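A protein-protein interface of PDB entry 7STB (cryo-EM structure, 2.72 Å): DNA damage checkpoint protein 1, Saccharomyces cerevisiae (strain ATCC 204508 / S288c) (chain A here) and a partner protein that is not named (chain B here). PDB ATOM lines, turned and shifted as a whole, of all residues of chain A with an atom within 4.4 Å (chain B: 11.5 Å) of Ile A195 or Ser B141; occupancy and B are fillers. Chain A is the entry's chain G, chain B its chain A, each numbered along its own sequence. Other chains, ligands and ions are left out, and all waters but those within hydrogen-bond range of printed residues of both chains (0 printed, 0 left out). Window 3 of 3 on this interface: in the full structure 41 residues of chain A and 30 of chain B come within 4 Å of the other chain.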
ATOM      1  N   PRO A 193       4.808 -13.995   4.231  1.00  0.00           N
ATOM      2  CA  PRO A 193       4.682 -12.573   3.892  1.00  0.00           C
ATOM      3  C   PRO A 193       5.035 -12.294   2.439  1.00  0.00           C
ATOM      4  O   PRO A 193       5.920 -12.925   1.856  1.00  0.00           O
ATOM      5  CB  PRO A 193       5.670 -11.889   4.847  1.00  0.00           C
ATOM      6  CG  PRO A 193       5.869 -12.859   5.958  1.00  0.00           C
ATOM      7  CD  PRO A 193       5.742 -14.215   5.348  1.00  0.00           C
ATOM      8  N   ILE A 194       4.323 -11.332   1.859  1.00  0.00           N
ATOM      9  CA  ILE A 194       4.567 -10.869   0.498  1.00  0.00           C
ATOM     10  C   ILE A 194       5.334  -9.558   0.581  1.00  0.00           C
ATOM     11  O   ILE A 194       4.899  -8.617   1.258  1.00  0.00           O
ATOM     12  CB  ILE A 194       3.249 -10.693  -0.276  1.00  0.00           C
ATOM     13  CG1 ILE A 194       2.425 -11.983  -0.228  1.00  0.00           C
ATOM     14  CG2 ILE A 194       3.519 -10.320  -1.727  1.00  0.00           C
ATOM     15  CD1 ILE A 194       1.035 -11.841  -0.808  1.00  0.00           C
ATOM     16  N   ILE A 195       6.474  -9.491  -0.105  1.00  0.00           N
ATOM     17  CA  ILE A 195       7.366  -8.342  -0.027  1.00  0.00           C
ATOM     18  C   ILE A 195       7.542  -7.671  -1.389  1.00  0.00           C
ATOM     19  O   ILE A 195       8.496  -6.929  -1.593  1.00  0.00           O
ATOM     20  CB  ILE A 195       8.727  -8.742   0.575  1.00  0.00           C
ATOM     21  CG1 ILE A 195       9.357  -9.878  -0.233  1.00  0.00           C
ATOM     22  CG2 ILE A 195       8.559  -9.155   2.029  1.00  0.00           C
ATOM     23  CD1 ILE A 195      10.789 -10.178   0.154  1.00  0.00           C
ATOM     24  N   ILE A 196       6.628  -7.920  -2.328  1.00  0.00           N
ATOM     25  CA  ILE A 196       6.706  -7.257  -3.627  1.00  0.00           C
ATOM     26  C   ILE A 196       6.563  -5.751  -3.458  1.00  0.00           C
ATOM     27  O   ILE A 196       7.249  -4.966  -4.125  1.00  0.00           O
ATOM     28  CB  ILE A 196       5.643  -7.828  -4.585  1.00  0.00           C
ATOM     29  CG1 ILE A 196       5.821  -7.255  -5.995  1.00  0.00           C
ATOM     30  CG2 ILE A 196       4.243  -7.526  -4.076  1.00  0.00           C
ATOM     31  CD1 ILE A 196       7.093  -7.700  -6.686  1.00  0.00           C
ATOM     32  N   ASN A 197       5.669  -5.323  -2.564  1.00  0.00           N
ATOM     33  CA  ASN A 197       5.503  -3.896  -2.312  1.00  0.00           C
ATOM     34  C   ASN A 197       6.781  -3.287  -1.751  1.00  0.00           C
ATOM     35  O   ASN A 197       7.142  -2.158  -2.101  1.00  0.00           O
ATOM     36  CB  ASN A 197       4.330  -3.661  -1.359  1.00  0.00           C
ATOM     37  CG  ASN A 197       4.441  -4.473  -0.085  1.00  0.00           C
ATOM     38  OD1 ASN A 197       5.400  -5.219   0.107  1.00  0.00           O
ATOM     39  ND2 ASN A 197       3.458  -4.330   0.794  1.00  0.00           N
ATOM     40  N   LEU A 198       7.477  -4.013  -0.875  1.00  0.00           N
ATOM     41  CA  LEU A 198       8.732  -3.505  -0.330  1.00  0.00           C
ATOM     42  C   LEU A 198       9.745  -3.263  -1.443  1.00  0.00           C
ATOM     43  O   LEU A 198      10.404  -2.217  -1.487  1.00  0.00           O
ATOM     44  CB  LEU A 198       9.291  -4.488   0.700  1.00  0.00           C
ATOM     45  CG  LEU A 198       8.790  -4.370   2.142  1.00  0.00           C
ATOM     46  CD1 LEU A 198       9.168  -3.029   2.750  1.00  0.00           C
ATOM     47  CD2 LEU A 198       7.288  -4.587   2.212  1.00  0.00           C
ATOM     48  N   LYS A 199       9.875  -4.224  -2.360  1.00  0.00           N
ATOM     49  CA  LYS A 199      10.819  -4.074  -3.462  1.00  0.00           C
ATOM     50  C   LYS A 199      10.418  -2.931  -4.385  1.00  0.00           C
ATOM     51  O   LYS A 199      11.278  -2.180  -4.859  1.00  0.00           O
ATOM     52  CB  LYS A 199      10.922  -5.385  -4.241  1.00  0.00           C
ATOM     53  CG  LYS A 199      11.415  -6.555  -3.406  1.00  0.00           C
ATOM     54  CD  LYS A 199      11.789  -7.745  -4.273  1.00  0.00           C
ATOM     55  CE  LYS A 199      12.481  -8.827  -3.458  1.00  0.00           C
ATOM     56  NZ  LYS A 199      12.869  -9.997  -4.292  1.00  0.00           N
ATOM     57  N   ARG B 131      10.702 -21.088 -18.085  1.00  0.00           N
ATOM     58  CA  ARG B 131      10.273 -19.943 -17.289  1.00  0.00           C
ATOM     59  C   ARG B 131      11.336 -18.853 -17.318  1.00  0.00           C
ATOM     60  O   ARG B 131      12.475 -19.071 -16.895  1.00  0.00           O
ATOM     61  CB  ARG B 131       9.993 -20.377 -15.851  1.00  0.00           C
ATOM     62  CG  ARG B 131       9.148 -19.393 -15.056  1.00  0.00           C
ATOM     63  CD  ARG B 131       8.435 -20.084 -13.904  1.00  0.00           C
ATOM     64  NE  ARG B 131       7.473 -19.211 -13.244  1.00  0.00           N
ATOM     65  CZ  ARG B 131       7.774 -18.344 -12.285  1.00  0.00           C
ATOM     66  NH1 ARG B 131       9.015 -18.195 -11.851  1.00  0.00           N
ATOM     67  NH2 ARG B 131       6.805 -17.608 -11.750  1.00  0.00           N
ATOM     68  N   SER B 134      13.115 -13.783 -13.359  1.00  0.00           N
ATOM     69  CA  SER B 134      12.538 -12.546 -12.857  1.00  0.00           C
ATOM     70  C   SER B 134      13.631 -11.615 -12.347  1.00  0.00           C
ATOM     71  O   SER B 134      14.767 -12.028 -12.092  1.00  0.00           O
ATOM     72  CB  SER B 134      11.532 -12.832 -11.739  1.00  0.00           C
ATOM     73  OG  SER B 134      12.169 -13.428 -10.623  1.00  0.00           O
ATOM     74  N   ASN B 135      13.270 -10.344 -12.199  1.00  0.00           N
ATOM     75  CA  ASN B 135      14.168  -9.302 -11.720  1.00  0.00           C
ATOM     76  C   ASN B 135      13.671  -8.736 -10.394  1.00  0.00           C
ATOM     77  O   ASN B 135      13.663  -7.523 -10.177  1.00  0.00           O
ATOM     78  CB  ASN B 135      14.314  -8.192 -12.757  1.00  0.00           C
ATOM     79  CG  ASN B 135      14.817  -8.706 -14.093  1.00  0.00           C
ATOM     80  OD1 ASN B 135      15.226  -9.860 -14.211  1.00  0.00           O
ATOM     81  ND2 ASN B 135      14.789  -7.847 -15.105  1.00  0.00           N
ATOM     82  N   GLY B 136      13.247  -9.618  -9.494  1.00  0.00           N
ATOM     83  CA  GLY B 136      12.682  -9.196  -8.229  1.00  0.00           C
ATOM     84  C   GLY B 136      11.205  -8.883  -8.271  1.00  0.00           C
ATOM     85  O   GLY B 136      10.712  -8.176  -7.384  1.00  0.00           O
ATOM     86  N   THR B 137      10.483  -9.383  -9.271  1.00  0.00           N
ATOM     87  CA  THR B 137       9.059  -9.126  -9.422  1.00  0.00           C
ATOM     88  C   THR B 137       8.198 -10.261  -8.882  1.00  0.00           C
ATOM     89  O   THR B 137       6.977 -10.244  -9.072  1.00  0.00           O
ATOM     90  CB  THR B 137       8.725  -8.878 -10.895  1.00  0.00           C
ATOM     91  OG1 THR B 137       9.074 -10.031 -11.671  1.00  0.00           O
ATOM     92  CG2 THR B 137       9.483  -7.665 -11.419  1.00  0.00           C
ATOM     93  N   SER B 138       8.800 -11.244  -8.219  1.00  0.00           N
ATOM     94  CA  SER B 138       8.039 -12.331  -7.624  1.00  0.00           C
ATOM     95  C   SER B 138       7.242 -11.828  -6.426  1.00  0.00           C
ATOM     96  O   SER B 138       7.663 -10.913  -5.711  1.00  0.00           O
ATOM     97  CB  SER B 138       8.968 -13.464  -7.191  1.00  0.00           C
ATOM     98  OG  SER B 138      10.010 -12.981  -6.361  1.00  0.00           O
ATOM     99  N   PHE B 139       6.074 -12.438  -6.214  1.00  0.00           N
ATOM    100  CA  PHE B 139       5.208 -12.041  -5.110  1.00  0.00           C
ATOM    101  C   PHE B 139       5.964 -12.050  -3.786  1.00  0.00           C
ATOM    102  O   PHE B 139       6.067 -11.026  -3.102  1.00  0.00           O
ATOM    103  CB  PHE B 139       3.996 -12.974  -5.040  1.00  0.00           C
ATOM    104  CG  PHE B 139       2.883 -12.596  -5.974  1.00  0.00           C
ATOM    105  CD1 PHE B 139       2.881 -13.035  -7.287  1.00  0.00           C
ATOM    106  CD2 PHE B 139       1.835 -11.804  -5.537  1.00  0.00           C
ATOM    107  CE1 PHE B 139       1.856 -12.689  -8.145  1.00  0.00           C
ATOM    108  CE2 PHE B 139       0.808 -11.455  -6.392  1.00  0.00           C
ATOM    109  CZ  PHE B 139       0.819 -11.897  -7.697  1.00  0.00           C
ATOM    110  N   ARG B 140       6.506 -13.204  -3.415  1.00  0.00           N
ATOM    111  CA  ARG B 140       7.208 -13.389  -2.155  1.00  0.00           C
ATOM    112  C   ARG B 140       8.682 -13.668  -2.414  1.00  0.00           C
ATOM    113  O   ARG B 140       9.123 -13.826  -3.556  1.00  0.00           O
ATOM    114  CB  ARG B 140       6.579 -14.534  -1.352  1.00  0.00           C
ATOM    115  CG  ARG B 140       5.082 -14.374  -1.115  1.00  0.00           C
ATOM    116  CD  ARG B 140       4.436 -15.686  -0.707  1.00  0.00           C
ATOM    117  NE  ARG B 140       2.981 -15.620  -0.768  1.00  0.00           N
ATOM    118  CZ  ARG B 140       2.174 -16.647  -0.539  1.00  0.00           C
ATOM    119  NH1 ARG B 140       2.647 -17.842  -0.223  1.00  0.00           N
ATOM    120  NH2 ARG B 140       0.858 -16.472  -0.630  1.00  0.00           N
ATOM    121  N   SER B 141       9.451 -13.726  -1.324  1.00  0.00           N
ATOM    122  CA  SER B 141      10.870 -14.042  -1.435  1.00  0.00           C
ATOM    123  C   SER B 141      11.102 -15.425  -2.027  1.00  0.00           C
ATOM    124  O   SER B 141      12.185 -15.684  -2.564  1.00  0.00           O
ATOM    125  CB  SER B 141      11.537 -13.944  -0.062  1.00  0.00           C
ATOM    126  OG  SER B 141      12.940 -14.109  -0.163  1.00  0.00           O
ATOM    127  N   THR B 142      10.117 -16.315  -1.941  1.00  0.00           N
ATOM    128  CA  THR B 142      10.250 -17.646  -2.501  1.00  0.00           C
ATOM    129  C   THR B 142      10.237 -17.582  -4.028  1.00  0.00           C
ATOM    130  O   THR B 142       9.778 -16.599  -4.615  1.00  0.00           O
ATOM    131  CB  THR B 142       9.122 -18.546  -2.006  1.00  0.00           C
ATOM    132  OG1 THR B 142       7.858 -17.937  -2.295  1.00  0.00           O
ATOM    133  CG2 THR B 142       9.243 -18.777  -0.505  1.00  0.00           C
ATOM    134  N   PRO B 143      10.740 -18.627  -4.697  1.00  0.00           N
ATOM    135  CA  PRO B 143      10.803 -18.597  -6.165  1.00  0.00           C
ATOM    136  C   PRO B 143       9.468 -18.881  -6.840  1.00  0.00           C
ATOM    137  O   PRO B 143       9.428 -19.142  -8.046  1.00  0.00           O
ATOM    138  CB  PRO B 143      11.834 -19.686  -6.487  1.00  0.00           C
ATOM    139  CG  PRO B 143      11.716 -20.647  -5.362  1.00  0.00           C
ATOM    140  CD  PRO B 143      11.396 -19.825  -4.142  1.00  0.00           C
ATOM    141  N   ASN B 144       8.371 -18.834  -6.082  1.00  0.00           N
ATOM    142  CA  ASN B 144       7.029 -19.061  -6.618  1.00  0.00           C
ATOM    143  C   ASN B 144       6.916 -20.463  -7.227  1.00  0.00           C
ATOM    144  O   ASN B 144       6.784 -20.649  -8.437  1.00  0.00           O
ATOM    145  CB  ASN B 144       6.664 -17.983  -7.648  1.00  0.00           C
ATOM    146  CG  ASN B 144       6.550 -16.602  -7.033  1.00  0.00           C
ATOM    147  OD1 ASN B 144       6.740 -16.428  -5.829  1.00  0.00           O
ATOM    148  ND2 ASN B 144       6.234 -15.611  -7.859  1.00  0.00           N
ATOM    149  N   GLU B 145       6.979 -21.453  -6.336  1.00  0.00           N
ATOM    150  CA  GLU B 145       6.880 -22.860  -6.723  1.00  0.00           C
ATOM    151  C   GLU B 145       5.428 -23.149  -7.102  1.00  0.00           C
ATOM    152  O   GLU B 145       4.638 -23.691  -6.328  1.00  0.00           O
ATOM    153  CB  GLU B 145       7.352 -23.760  -5.587  1.00  0.00           C
ATOM    154  CG  GLU B 145       7.276 -25.249  -5.892  1.00  0.00           C
ATOM    155  CD  GLU B 145       7.663 -26.107  -4.704  1.00  0.00           C
ATOM    156  OE1 GLU B 145       7.935 -25.540  -3.624  1.00  0.00           O
ATOM    157  OE2 GLU B 145       7.695 -27.346  -4.848  1.00  0.00           O
ATOM    158  N   HIS B 146       5.080 -22.769  -8.329  1.00  0.00           N
ATOM    159  CA  HIS B 146       3.724 -22.912  -8.853  1.00  0.00           C
ATOM    160  C   HIS B 146       3.772 -23.479 -10.268  1.00  0.00           C
ATOM    161  O   HIS B 146       3.153 -22.957 -11.195  1.00  0.00           O
ATOM    162  CB  HIS B 146       2.990 -21.572  -8.823  1.00  0.00           C
ATOM    163  CG  HIS B 146       2.864 -20.983  -7.452  1.00  0.00           C
ATOM    164  ND1 HIS B 146       3.761 -20.064  -6.952  1.00  0.00           N
ATOM    165  CD2 HIS B 146       1.947 -21.182  -6.477  1.00  0.00           C
ATOM    166  CE1 HIS B 146       3.402 -19.722  -5.727  1.00  0.00           C
ATOM    167  NE2 HIS B 146       2.304 -20.387  -5.415  1.00  0.00           N
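The backbone NH (N) of Ile A196 lies within hydrogen-bond range of the backbone carbonyl oxygen (O) of Phe B139, at 3.2 Å.
N of Ile A195 is in hydrogen-bond range of O of Phe B139 (3.4 Å).
The backbone carbonyl oxygen (O) of Arg B140 sits at hydrogen-bond distance from the side-chain hydroxyl (OG) of Ser B138.
Pro A193 touches Arg B140.
CG2 of Ile A194 touches O of Phe B139 (3.0 Å).
Ile A194 touches Arg B140.
Ile A195 touches Ser B141 (CD1 to CB, 3.8 Å).
Ile A196 touches Gly B136.
Thr B137 touches Ile A196.
Ile A196 touches Ser B138.
O of Gly B136 touches CD of Lys A199, 3.3 Å away.
Pro A193 touches just one residue of chain B: Arg B140 (3.4 Å).
Of chain B, only Phe B139 (3.0 Å) and Arg B140 (3.7 Å) come within 4 Å of Ile A194.
Of chain B, only Phe B139 (3.4 Å) and Ser B141 (3.8 Å) come within 4 Å of Ile A195.
Ile A196 touches just these residues of chain B: Gly B136, Thr B137, Ser B138 and Phe B139.
No residue of chain B comes within 4 Å of Asn A197.
No residue of chain B comes within 4 Å of Leu A198.
Lys A199 touches just one residue of chain B: Gly B136.
Of the printed residues of chain A, Gly B136 touches Ile A196 and Lys A199.
Of the printed residues of chain A, Thr B137 touches Ile A196.
Of the printed residues of chain A, Phe B139 touches Ile A194, Ile A195 and Ile A196.
Ser B141 touches just one residue of chain A: Ile A195.
His B146 touches none of the printed residues of chain A.
Along chain A the printed residues that touch a printed residue of chain B span positions 193 to 199.
Along chain B the printed residues that touch a printed residue of chain A span positions 136 to 141.
Among the printed residues, no Asp or Glu carboxylate lies within 4 Å of a Lys or Arg side-chain nitrogen of the other chain.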
